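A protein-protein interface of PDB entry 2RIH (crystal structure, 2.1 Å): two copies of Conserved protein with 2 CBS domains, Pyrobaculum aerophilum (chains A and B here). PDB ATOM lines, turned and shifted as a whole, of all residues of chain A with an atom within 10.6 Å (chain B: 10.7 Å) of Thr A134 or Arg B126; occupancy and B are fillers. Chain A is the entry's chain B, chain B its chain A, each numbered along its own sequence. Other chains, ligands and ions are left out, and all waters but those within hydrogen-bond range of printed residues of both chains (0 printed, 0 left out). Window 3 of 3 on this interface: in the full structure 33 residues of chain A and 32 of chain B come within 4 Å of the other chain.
The backbone carbonyl oxygen of Leu A130 lies within hydrogen-bond range of the side-chain hydroxyl of Thr A134 (3.2 Å).
O of Leu B130 sits at hydrogen-bond distance from OG1 of Thr B134.
Of the 19 printed residues of chain A, 9 touch a printed residue of chain B.
Along chain A the printed residues that touch a printed residue of chain B span positions 97 to 134.
Among the printed residues, 15 pairs touch across the chains.
Among the printed residues, no Asp or Glu carboxylate lies within 4 Å of a Lys or Arg side-chain nitrogen of the other chain.
Cys A123 touches its own counterpart, Cys B123.
Leu A129 touches Leu B132, and with the chains exchanged Leu A132 touches Leu B129.
Leu A130 touches Ala B133, and with the chains exchanged Ala A133 touches Leu B130.
Thr A134 touches Arg B126, but with the chains exchanged Arg A126 does not touch Thr B134 (5.5 Å).
Positions printed for both chains: 5, 89, 123, 126, 127, 128, 129, 130, 131, 132, 133 and 134.
Of the printed residues of chain B, Arg A97 touches Phe B124 (3.3 Å).
Of the printed residues of chain B, Cys A123 touches Cys B123 (2.0 Å) and Leu B132 (3.8 Å).
Of the printed residues of chain B, Leu A132 touches Arg B126 and Leu B129.
Ala A133 touches two residues of chain B.
Thr A134 touches one residue of chain B.
Arg B126 touches three residues of chain A.
No residue of chain A comes within 4 Å of Ala B127.
No residue of chain A comes within 4 Å of Ile B128.
Leu B129 touches two residues of chain A.
Of chain A, only Ala A133 (3.8 Å) comes within 4 Å of Leu B130.
Glu B131 touches none of the printed residues of chain A.
Printed residues of chain A within 4 Å of Ala B133: Arg A126 (3.3 Å), Leu A129 (3.9 Å) and Leu A130 (3.6 Å).
The nearest printed residue of chain A that does not touch Arg B126 is Arg A97 (4.7 Å).
O of Leu A132 lies within hydrogen-bond range of NE of Arg B126 (3.1 Å).
The side-chain sulfur of Cys B123 forms a disulfide with the side-chain sulfur of Cys A123.
NE of Arg A97 sits at hydrogen-bond distance from O of Phe B124 (3.3 Å).
Among the printed residues, merely in contact across the chains: Ala A133 with Arg B126 (3.3 Å), Arg A126 with Ala B133 (3.3 Å), Thr A134 with Arg B126 (3.4 Å), Leu A129 with Leu B129 (3.5 Å), Ile A119 with Cys B123 (3.5 Å), Leu A130 with Ala B133 (3.6 Å), Ala A133 with Leu B130 (3.8 Å), Cys A123 with Leu B132 (3.8 Å), Leu A132 with Leu B129 (3.8 Å), Ile A119 with Phe B124 (3.8 Å), Leu A129 with Leu B132 (3.9 Å) and Leu A129 with Ala B133 (3.9 Å).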
ATOM      1  N   ILE A   5     -19.047  26.961  16.062  1.00  0.00           N
ATOM      2  CA  ILE A   5     -20.320  26.288  16.460  1.00  0.00           C
ATOM      3  C   ILE A   5     -21.439  27.324  16.558  1.00  0.00           C
ATOM      4  O   ILE A   5     -21.259  28.383  17.169  1.00  0.00           O
ATOM      5  CB  ILE A   5     -20.187  25.563  17.827  1.00  0.00           C
ATOM      6  CG1 ILE A   5     -18.978  24.619  17.837  1.00  0.00           C
ATOM      7  CG2 ILE A   5     -21.447  24.772  18.139  1.00  0.00           C
ATOM      8  CD1 ILE A   5     -18.612  24.112  19.222  1.00  0.00           C
ATOM      9  N   VAL A  89     -21.940  30.398  19.114  1.00  0.00           N
ATOM     10  CA  VAL A  89     -22.172  30.131  20.530  1.00  0.00           C
ATOM     11  C   VAL A  89     -21.493  31.133  21.470  1.00  0.00           C
ATOM     12  O   VAL A  89     -21.978  31.337  22.588  1.00  0.00           O
ATOM     13  CB  VAL A  89     -21.786  28.666  20.905  1.00  0.00           C
ATOM     14  CG1 VAL A  89     -21.688  28.489  22.409  1.00  0.00           C
ATOM     15  CG2 VAL A  89     -22.816  27.694  20.351  1.00  0.00           C
ATOM     16  N   HIS A  90     -20.394  31.760  21.039  1.00  0.00           N
ATOM     17  CA  HIS A  90     -19.737  32.785  21.879  1.00  0.00           C
ATOM     18  C   HIS A  90     -20.667  33.969  22.186  1.00  0.00           C
ATOM     19  O   HIS A  90     -20.551  34.584  23.247  1.00  0.00           O
ATOM     20  CB  HIS A  90     -18.393  33.266  21.301  1.00  0.00           C
ATOM     21  CG  HIS A  90     -18.509  34.194  20.126  1.00  0.00           C
ATOM     22  ND1 HIS A  90     -18.358  33.771  18.821  1.00  0.00           N
ATOM     23  CD2 HIS A  90     -18.720  35.529  20.062  1.00  0.00           C
ATOM     24  CE1 HIS A  90     -18.494  34.802  18.006  1.00  0.00           C
ATOM     25  NE2 HIS A  90     -18.713  35.882  18.735  1.00  0.00           N
ATOM     26  N   VAL A  91     -21.588  34.274  21.271  1.00  0.00           N
ATOM     27  CA  VAL A  91     -22.568  35.334  21.497  1.00  0.00           C
ATOM     28  C   VAL A  91     -23.523  34.936  22.626  1.00  0.00           C
ATOM     29  O   VAL A  91     -23.863  35.765  23.481  1.00  0.00           O
ATOM     30  CB  VAL A  91     -23.362  35.693  20.204  1.00  0.00           C
ATOM     31  CG1 VAL A  91     -24.579  36.557  20.531  1.00  0.00           C
ATOM     32  CG2 VAL A  91     -22.462  36.418  19.211  1.00  0.00           C
ATOM     33  N   ALA A  93     -22.835  32.864  25.130  1.00  0.00           N
ATOM     34  CA  ALA A  93     -22.021  32.944  26.345  1.00  0.00           C
ATOM     35  C   ALA A  93     -21.828  34.391  26.819  1.00  0.00           C
ATOM     36  O   ALA A  93     -21.821  34.664  28.015  1.00  0.00           O
ATOM     37  CB  ALA A  93     -20.650  32.282  26.106  1.00  0.00           C
ATOM     38  N   GLU A  94     -21.653  35.303  25.868  1.00  0.00           N
ATOM     39  CA  GLU A  94     -21.512  36.721  26.168  1.00  0.00           C
ATOM     40  C   GLU A  94     -22.761  37.305  26.811  1.00  0.00           C
ATOM     41  O   GLU A  94     -22.665  38.044  27.772  1.00  0.00           O
ATOM     42  CB  GLU A  94     -21.161  37.498  24.901  1.00  0.00           C
ATOM     43  CG  GLU A  94     -19.715  37.324  24.474  1.00  0.00           C
ATOM     44  CD  GLU A  94     -19.496  37.568  22.993  1.00  0.00           C
ATOM     45  OE1 GLU A  94     -20.408  38.085  22.317  1.00  0.00           O
ATOM     46  OE2 GLU A  94     -18.392  37.247  22.508  1.00  0.00           O
ATOM     47  N   ARG A  97     -23.266  35.976  30.459  1.00  0.00           N
ATOM     48  CA  ARG A  97     -22.237  36.598  31.272  1.00  0.00           C
ATOM     49  C   ARG A  97     -22.563  38.063  31.578  1.00  0.00           C
ATOM     50  O   ARG A  97     -22.552  38.496  32.732  1.00  0.00           O
ATOM     51  CB  ARG A  97     -20.935  36.484  30.470  1.00  0.00           C
ATOM     52  CG  ARG A  97     -19.687  37.100  31.038  1.00  0.00           C
ATOM     53  CD  ARG A  97     -18.610  37.077  29.965  1.00  0.00           C
ATOM     54  NE  ARG A  97     -18.440  35.741  29.394  1.00  0.00           N
ATOM     55  CZ  ARG A  97     -17.898  35.471  28.204  1.00  0.00           C
ATOM     56  NH1 ARG A  97     -17.458  36.442  27.408  1.00  0.00           N
ATOM     57  NH2 ARG A  97     -17.806  34.207  27.802  1.00  0.00           N
ATOM     58  N   ARG A  98     -22.874  38.809  30.525  1.00  0.00           N
ATOM     59  CA  ARG A  98     -23.109  40.252  30.610  1.00  0.00           C
ATOM     60  C   ARG A  98     -24.464  40.622  31.209  1.00  0.00           C
ATOM     61  O   ARG A  98     -24.588  41.669  31.834  1.00  0.00           O
ATOM     62  CB  ARG A  98     -22.888  40.890  29.242  1.00  0.00           C
ATOM     63  CG  ARG A  98     -21.442  40.772  28.812  1.00  0.00           C
ATOM     64  CD  ARG A  98     -21.217  41.123  27.361  1.00  0.00           C
ATOM     65  NE  ARG A  98     -19.852  40.791  26.948  1.00  0.00           N
ATOM     66  CZ  ARG A  98     -19.384  40.933  25.710  1.00  0.00           C
ATOM     67  NH1 ARG A  98     -20.161  41.380  24.742  1.00  0.00           N
ATOM     68  NH2 ARG A  98     -18.123  40.629  25.439  1.00  0.00           N
ATOM     69  N   ILE A 119     -26.191  27.586  30.428  1.00  0.00           N
ATOM     70  CA  ILE A 119     -24.740  27.683  30.675  1.00  0.00           C
ATOM     71  C   ILE A 119     -24.145  26.278  30.854  1.00  0.00           C
ATOM     72  O   ILE A 119     -22.994  26.019  30.476  1.00  0.00           O
ATOM     73  CB  ILE A 119     -24.419  28.601  31.890  1.00  0.00           C
ATOM     74  CG1 ILE A 119     -22.905  28.846  32.020  1.00  0.00           C
ATOM     75  CG2 ILE A 119     -24.999  28.024  33.186  1.00  0.00           C
ATOM     76  CD1 ILE A 119     -22.255  29.498  30.798  1.00  0.00           C
ATOM     77  N   CYS A 123     -20.568  24.824  29.087  1.00  0.00           N
ATOM     78  CA  CYS A 123     -19.401  24.764  29.969  1.00  0.00           C
ATOM     79  C   CYS A 123     -18.692  23.418  30.141  1.00  0.00           C
ATOM     80  O   CYS A 123     -17.580  23.381  30.652  1.00  0.00           O
ATOM     81  CB  CYS A 123     -19.819  25.239  31.354  1.00  0.00           C
ATOM     82  SG  CYS A 123     -18.472  25.707  32.432  1.00  0.00           S
ATOM     83  N   ARG A 126     -15.249  19.923  26.065  1.00  0.00           N
ATOM     84  CA  ARG A 126     -13.945  20.550  25.795  1.00  0.00           C
ATOM     85  C   ARG A 126     -13.961  21.421  24.530  1.00  0.00           C
ATOM     86  O   ARG A 126     -13.392  22.518  24.522  1.00  0.00           O
ATOM     87  CB  ARG A 126     -12.827  19.492  25.717  1.00  0.00           C
ATOM     88  CG  ARG A 126     -11.580  19.955  24.957  1.00  0.00           C
ATOM     89  CD  ARG A 126     -10.272  19.410  25.512  1.00  0.00           C
ATOM     90  NE  ARG A 126      -9.947  18.042  25.113  1.00  0.00           N
ATOM     91  CZ  ARG A 126      -9.563  17.662  23.892  1.00  0.00           C
ATOM     92  NH1 ARG A 126      -9.493  18.535  22.893  1.00  0.00           N
ATOM     93  NH2 ARG A 126      -9.272  16.388  23.659  1.00  0.00           N
ATOM     94  N   ALA A 127     -14.620  20.932  23.479  1.00  0.00           N
ATOM     95  CA  ALA A 127     -14.664  21.620  22.180  1.00  0.00           C
ATOM     96  C   ALA A 127     -15.397  22.957  22.262  1.00  0.00           C
ATOM     97  O   ALA A 127     -14.985  23.938  21.636  1.00  0.00           O
ATOM     98  CB  ALA A 127     -15.314  20.727  21.130  1.00  0.00           C
ATOM     99  N   ILE A 128     -16.482  22.989  23.031  1.00  0.00           N
ATOM    100  CA  ILE A 128     -17.234  24.226  23.254  1.00  0.00           C
ATOM    101  C   ILE A 128     -16.420  25.135  24.174  1.00  0.00           C
ATOM    102  O   ILE A 128     -16.266  26.324  23.894  1.00  0.00           O
ATOM    103  CB  ILE A 128     -18.618  23.977  23.874  1.00  0.00           C
ATOM    104  CG1 ILE A 128     -19.420  22.951  23.065  1.00  0.00           C
ATOM    105  CG2 ILE A 128     -19.412  25.285  23.943  1.00  0.00           C
ATOM    106  CD1 ILE A 128     -20.758  22.608  23.699  1.00  0.00           C
ATOM    107  N   LEU A 129     -15.892  24.559  25.259  1.00  0.00           N
ATOM    108  CA  LEU A 129     -15.026  25.269  26.207  1.00  0.00           C
ATOM    109  C   LEU A 129     -13.850  25.951  25.526  1.00  0.00           C
ATOM    110  O   LEU A 129     -13.577  27.125  25.791  1.00  0.00           O
ATOM    111  CB  LEU A 129     -14.465  24.318  27.280  1.00  0.00           C
ATOM    112  CG  LEU A 129     -15.306  23.994  28.511  1.00  0.00           C
ATOM    113  CD1 LEU A 129     -14.610  22.915  29.332  1.00  0.00           C
ATOM    114  CD2 LEU A 129     -15.565  25.252  29.346  1.00  0.00           C
ATOM    115  N   LEU A 130     -13.143  25.203  24.676  1.00  0.00           N
ATOM    116  CA  LEU A 130     -11.972  25.735  23.973  1.00  0.00           C
ATOM    117  C   LEU A 130     -12.377  26.846  23.013  1.00  0.00           C
ATOM    118  O   LEU A 130     -11.677  27.848  22.897  1.00  0.00           O
ATOM    119  CB  LEU A 130     -11.198  24.628  23.238  1.00  0.00           C
ATOM    120  CG  LEU A 130     -10.276  23.749  24.099  1.00  0.00           C
ATOM    121  CD1 LEU A 130      -9.808  22.530  23.323  1.00  0.00           C
ATOM    122  CD2 LEU A 130      -9.077  24.536  24.624  1.00  0.00           C
ATOM    123  N   GLU A 131     -13.516  26.676  22.348  1.00  0.00           N
ATOM    124  CA  GLU A 131     -14.056  27.719  21.470  1.00  0.00           C
ATOM    125  C   GLU A 131     -14.371  29.000  22.248  1.00  0.00           C
ATOM    126  O   GLU A 131     -13.987  30.101  21.831  1.00  0.00           O
ATOM    127  CB  GLU A 131     -15.299  27.219  20.727  1.00  0.00           C
ATOM    128  CG  GLU A 131     -15.909  28.250  19.788  1.00  0.00           C
ATOM    129  CD  GLU A 131     -16.763  27.631  18.687  1.00  0.00           C
ATOM    130  OE1 GLU A 131     -16.233  26.810  17.897  1.00  0.00           O
ATOM    131  OE2 GLU A 131     -17.956  27.986  18.599  1.00  0.00           O
ATOM    132  N   LEU A 132     -15.061  28.853  23.377  1.00  0.00           N
ATOM    133  CA  LEU A 132     -15.365  29.993  24.251  1.00  0.00           C
ATOM    134  C   LEU A 132     -14.119  30.551  24.952  1.00  0.00           C
ATOM    135  O   LEU A 132     -14.064  31.739  25.265  1.00  0.00           O
ATOM    136  CB  LEU A 132     -16.407  29.607  25.304  1.00  0.00           C
ATOM    137  CG  LEU A 132     -17.782  29.172  24.791  1.00  0.00           C
ATOM    138  CD1 LEU A 132     -18.701  28.835  25.961  1.00  0.00           C
ATOM    139  CD2 LEU A 132     -18.390  30.247  23.922  1.00  0.00           C
ATOM    140  N   ALA A 133     -13.133  29.691  25.198  1.00  0.00           N
ATOM    141  CA  ALA A 133     -11.896  30.090  25.878  1.00  0.00           C
ATOM    142  C   ALA A 133     -10.998  30.992  25.025  1.00  0.00           C
ATOM    143  O   ALA A 133     -10.173  31.730  25.568  1.00  0.00           O
ATOM    144  CB  ALA A 133     -11.115  28.853  26.325  1.00  0.00           C
ATOM    145  N   THR A 134     -11.165  30.933  23.702  1.00  0.00           N
ATOM    146  CA  THR A 134     -10.309  31.665  22.766  1.00  0.00           C
ATOM    147  C   THR A 134     -11.106  32.685  21.947  1.00  0.00           C
ATOM    148  O   THR A 134     -10.540  33.423  21.131  1.00  0.00           O
ATOM    149  CB  THR A 134      -9.586  30.687  21.808  1.00  0.00           C
ATOM    150  OG1 THR A 134     -10.539  30.063  20.934  1.00  0.00           O
ATOM    151  CG2 THR A 134      -8.847  29.609  22.598  1.00  0.00           C
ATOM    152  N   ILE B   5      -5.996  27.468  39.475  1.00  0.00           N
ATOM    153  CA  ILE B   5      -7.066  28.208  40.213  1.00  0.00           C
ATOM    154  C   ILE B   5      -7.797  27.248  41.157  1.00  0.00           C
ATOM    155  O   ILE B   5      -8.238  26.177  40.738  1.00  0.00           O
ATOM    156  CB  ILE B   5      -8.075  28.877  39.254  1.00  0.00           C
ATOM    157  CG1 ILE B   5      -7.354  29.862  38.325  1.00  0.00           C
ATOM    158  CG2 ILE B   5      -9.175  29.587  40.042  1.00  0.00           C
ATOM    159  CD1 ILE B   5      -8.242  30.499  37.265  1.00  0.00           C
ATOM    160  N   LEU B  10     -12.789  31.590  43.985  1.00  0.00           N
ATOM    161  CA  LEU B  10     -14.009  32.000  43.287  1.00  0.00           C
ATOM    162  C   LEU B  10     -15.218  32.146  44.209  1.00  0.00           C
ATOM    163  O   LEU B  10     -16.330  32.342  43.735  1.00  0.00           O
ATOM    164  CB  LEU B  10     -14.344  30.995  42.185  1.00  0.00           C
ATOM    165  CG  LEU B  10     -13.210  30.646  41.218  1.00  0.00           C
ATOM    166  CD1 LEU B  10     -13.707  29.664  40.170  1.00  0.00           C
ATOM    167  CD2 LEU B  10     -12.604  31.904  40.557  1.00  0.00           C
ATOM    168  N   VAL B  89     -10.332  24.139  40.347  1.00  0.00           N
ATOM    169  CA  VAL B  89     -11.701  24.332  39.888  1.00  0.00           C
ATOM    170  C   VAL B  89     -12.203  23.232  38.932  1.00  0.00           C
ATOM    171  O   VAL B  89     -13.413  23.033  38.823  1.00  0.00           O
ATOM    172  CB  VAL B  89     -11.888  25.737  39.264  1.00  0.00           C
ATOM    173  CG1 VAL B  89     -11.612  26.818  40.312  1.00  0.00           C
ATOM    174  CG2 VAL B  89     -10.995  25.923  38.047  1.00  0.00           C
ATOM    175  N   ARG B 120     -22.179  29.292  37.589  1.00  0.00           N
ATOM    176  CA  ARG B 120     -21.924  30.703  37.224  1.00  0.00           C
ATOM    177  C   ARG B 120     -20.498  31.141  37.498  1.00  0.00           C
ATOM    178  O   ARG B 120     -19.927  31.930  36.735  1.00  0.00           O
ATOM    179  CB  ARG B 120     -22.788  31.636  38.056  1.00  0.00           C
ATOM    180  CG  ARG B 120     -24.121  31.975  37.514  1.00  0.00           C
ATOM    181  CD  ARG B 120     -24.905  32.677  38.620  1.00  0.00           C
ATOM    182  NE  ARG B 120     -25.766  33.694  38.069  1.00  0.00           N
ATOM    183  CZ  ARG B 120     -27.087  33.711  38.102  1.00  0.00           C
ATOM    184  NH1 ARG B 120     -27.807  32.771  38.703  1.00  0.00           N
ATOM    185  NH2 ARG B 120     -27.684  34.727  37.521  1.00  0.00           N
ATOM    186  N   ASP B 121     -19.950  30.672  38.617  1.00  0.00           N
ATOM    187  CA  ASP B 121     -18.602  31.051  39.051  1.00  0.00           C
ATOM    188  C   ASP B 121     -17.512  30.475  38.152  1.00  0.00           C
ATOM    189  O   ASP B 121     -16.431  31.062  38.008  1.00  0.00           O
ATOM    190  CB  ASP B 121     -18.358  30.589  40.490  1.00  0.00           C
ATOM    191  CG  ASP B 121     -19.328  31.208  41.483  1.00  0.00           C
ATOM    192  OD1 ASP B 121     -19.430  32.459  41.524  1.00  0.00           O
ATOM    193  OD2 ASP B 121     -19.971  30.442  42.248  1.00  0.00           O
ATOM    194  N   LEU B 122     -17.798  29.323  37.551  1.00  0.00           N
ATOM    195  CA  LEU B 122     -16.809  28.590  36.774  1.00  0.00           C
ATOM    196  C   LEU B 122     -16.852  28.869  35.281  1.00  0.00           C
ATOM    197  O   LEU B 122     -15.842  28.723  34.589  1.00  0.00           O
ATOM    198  CB  LEU B 122     -17.032  27.087  36.960  1.00  0.00           C
ATOM    199  CG  LEU B 122     -16.852  26.493  38.348  1.00  0.00           C
ATOM    200  CD1 LEU B 122     -17.228  25.026  38.328  1.00  0.00           C
ATOM    201  CD2 LEU B 122     -15.422  26.688  38.827  1.00  0.00           C
ATOM    202  N   CYS B 123     -18.020  29.249  34.777  1.00  0.00           N
ATOM    203  CA  CYS B 123     -18.276  29.139  33.346  1.00  0.00           C
ATOM    204  C   CYS B 123     -18.296  30.438  32.550  1.00  0.00           C
ATOM    205  O   CYS B 123     -18.526  30.403  31.342  1.00  0.00           O
ATOM    206  CB  CYS B 123     -19.574  28.369  33.150  1.00  0.00           C
ATOM    207  SG  CYS B 123     -19.464  26.730  33.856  1.00  0.00           S
ATOM    208  N   PHE B 124     -18.032  31.566  33.207  1.00  0.00           N
ATOM    209  CA  PHE B 124     -18.028  32.865  32.523  1.00  0.00           C
ATOM    210  C   PHE B 124     -16.626  33.375  32.132  1.00  0.00           C
ATOM    211  O   PHE B 124     -16.400  33.755  30.977  1.00  0.00           O
ATOM    212  CB  PHE B 124     -18.756  33.915  33.372  1.00  0.00           C
ATOM    213  CG  PHE B 124     -20.263  33.731  33.450  1.00  0.00           C
ATOM    214  CD1 PHE B 124     -20.973  33.021  32.481  1.00  0.00           C
ATOM    215  CD2 PHE B 124     -20.979  34.337  34.474  1.00  0.00           C
ATOM    216  CE1 PHE B 124     -22.359  32.882  32.565  1.00  0.00           C
ATOM    217  CE2 PHE B 124     -22.370  34.216  34.558  1.00  0.00           C
ATOM    218  CZ  PHE B 124     -23.056  33.480  33.602  1.00  0.00           C
ATOM    219  N   GLU B 125     -15.685  33.385  33.073  1.00  0.00           N
ATOM    220  CA  GLU B 125     -14.366  33.965  32.803  1.00  0.00           C
ATOM    221  C   GLU B 125     -13.468  33.054  31.958  1.00  0.00           C
ATOM    222  O   GLU B 125     -13.305  31.875  32.259  1.00  0.00           O
ATOM    223  CB  GLU B 125     -13.656  34.320  34.104  1.00  0.00           C
ATOM    224  CG  GLU B 125     -12.394  35.116  33.876  1.00  0.00           C
ATOM    225  CD  GLU B 125     -11.636  35.418  35.146  1.00  0.00           C
ATOM    226  OE1 GLU B 125     -12.188  35.221  36.247  1.00  0.00           O
ATOM    227  OE2 GLU B 125     -10.475  35.844  35.025  1.00  0.00           O
ATOM    228  N   ARG B 126     -12.864  33.633  30.921  1.00  0.00           N
ATOM    229  CA  ARG B 126     -12.054  32.884  29.955  1.00  0.00           C
ATOM    230  C   ARG B 126     -10.923  32.087  30.562  1.00  0.00           C
ATOM    231  O   ARG B 126     -10.749  30.920  30.226  1.00  0.00           O
ATOM    232  CB  ARG B 126     -11.460  33.810  28.884  1.00  0.00           C
ATOM    233  CG  ARG B 126     -12.051  33.623  27.503  1.00  0.00           C
ATOM    234  CD  ARG B 126     -13.137  34.630  27.153  1.00  0.00           C
ATOM    235  NE  ARG B 126     -13.301  34.680  25.701  1.00  0.00           N
ATOM    236  CZ  ARG B 126     -12.431  35.230  24.857  1.00  0.00           C
ATOM    237  NH1 ARG B 126     -11.314  35.807  25.305  1.00  0.00           N
ATOM    238  NH2 ARG B 126     -12.674  35.206  23.548  1.00  0.00           N
ATOM    239  N   ALA B 127     -10.137  32.735  31.421  1.00  0.00           N
ATOM    240  CA  ALA B 127      -9.024  32.086  32.109  1.00  0.00           C
ATOM    241  C   ALA B 127      -9.480  30.828  32.837  1.00  0.00           C
ATOM    242  O   ALA B 127      -8.743  29.838  32.916  1.00  0.00           O
ATOM    243  CB  ALA B 127      -8.370  33.051  33.097  1.00  0.00           C
ATOM    244  N   ILE B 128     -10.699  30.870  33.367  1.00  0.00           N
ATOM    245  CA  ILE B 128     -11.259  29.731  34.088  1.00  0.00           C
ATOM    246  C   ILE B 128     -11.689  28.653  33.076  1.00  0.00           C
ATOM    247  O   ILE B 128     -11.345  27.487  33.235  1.00  0.00           O
ATOM    248  CB  ILE B 128     -12.430  30.153  35.009  1.00  0.00           C
ATOM    249  CG1 ILE B 128     -11.993  31.295  35.951  1.00  0.00           C
ATOM    250  CG2 ILE B 128     -12.919  28.957  35.809  1.00  0.00           C
ATOM    251  CD1 ILE B 128     -13.069  31.798  36.881  1.00  0.00           C
ATOM    252  N   LEU B 129     -12.420  29.055  32.038  1.00  0.00           N
ATOM    253  CA  LEU B 129     -12.796  28.150  30.944  1.00  0.00           C
ATOM    254  C   LEU B 129     -11.575  27.438  30.358  1.00  0.00           C
ATOM    255  O   LEU B 129     -11.605  26.232  30.102  1.00  0.00           O
ATOM    256  CB  LEU B 129     -13.514  28.916  29.820  1.00  0.00           C
ATOM    257  CG  LEU B 129     -14.884  29.515  30.133  1.00  0.00           C
ATOM    258  CD1 LEU B 129     -15.458  30.218  28.912  1.00  0.00           C
ATOM    259  CD2 LEU B 129     -15.847  28.450  30.631  1.00  0.00           C
ATOM    260  N   LEU B 130     -10.502  28.197  30.158  1.00  0.00           N
ATOM    261  CA  LEU B 130      -9.263  27.667  29.592  1.00  0.00           C
ATOM    262  C   LEU B 130      -8.736  26.563  30.503  1.00  0.00           C
ATOM    263  O   LEU B 130      -8.391  25.474  30.046  1.00  0.00           O
ATOM    264  CB  LEU B 130      -8.236  28.799  29.448  1.00  0.00           C
ATOM    265  CG  LEU B 130      -7.038  28.620  28.522  1.00  0.00           C
ATOM    266  CD1 LEU B 130      -7.464  28.434  27.077  1.00  0.00           C
ATOM    267  CD2 LEU B 130      -6.119  29.822  28.651  1.00  0.00           C
ATOM    268  N   GLU B 131      -8.737  26.838  31.802  1.00  0.00           N
ATOM    269  CA  GLU B 131      -8.276  25.880  32.791  1.00  0.00           C
ATOM    270  C   GLU B 131      -9.186  24.645  32.872  1.00  0.00           C
ATOM    271  O   GLU B 131      -8.693  23.529  33.040  1.00  0.00           O
ATOM    272  CB  GLU B 131      -8.139  26.559  34.154  1.00  0.00           C
ATOM    273  CG  GLU B 131      -7.147  25.890  35.049  1.00  0.00           C
ATOM    274  CD  GLU B 131      -6.821  26.713  36.264  1.00  0.00           C
ATOM    275  OE1 GLU B 131      -6.142  27.747  36.104  1.00  0.00           O
ATOM    276  OE2 GLU B 131      -7.229  26.310  37.374  1.00  0.00           O
ATOM    277  N   LEU B 132     -10.499  24.834  32.734  1.00  0.00           N
ATOM    278  CA  LEU B 132     -11.418  23.696  32.616  1.00  0.00           C
ATOM    279  C   LEU B 132     -11.155  22.879  31.342  1.00  0.00           C
ATOM    280  O   LEU B 132     -11.292  21.661  31.347  1.00  0.00           O
ATOM    281  CB  LEU B 132     -12.888  24.148  32.614  1.00  0.00           C
ATOM    282  CG  LEU B 132     -13.449  24.892  33.825  1.00  0.00           C
ATOM    283  CD1 LEU B 132     -14.946  25.134  33.623  1.00  0.00           C
ATOM    284  CD2 LEU B 132     -13.194  24.141  35.124  1.00  0.00           C
ATOM    285  N   ALA B 133     -10.793  23.550  30.252  1.00  0.00           N
ATOM    286  CA  ALA B 133     -10.590  22.875  28.966  1.00  0.00           C
ATOM    287  C   ALA B 133      -9.299  22.042  28.920  1.00  0.00           C
ATOM    288  O   ALA B 133      -9.237  21.027  28.229  1.00  0.00           O
ATOM    289  CB  ALA B 133     -10.599  23.886  27.847  1.00  0.00           C
ATOM    290  N   THR B 134      -8.280  22.478  29.661  1.00  0.00           N
ATOM    291  CA  THR B 134      -6.974  21.819  29.684  1.00  0.00           C
ATOM    292  C   THR B 134      -6.986  20.480  30.428  1.00  0.00           C
ATOM    293  O   THR B 134      -6.319  19.527  30.010  1.00  0.00           O
ATOM    294  CB  THR B 134      -5.926  22.721  30.355  1.00  0.00           C
ATOM    295  OG1 THR B 134      -5.996  24.034  29.790  1.00  0.00           O
ATOM    296  CG2 THR B 134      -4.519  22.147  30.168  1.00  0.00           C
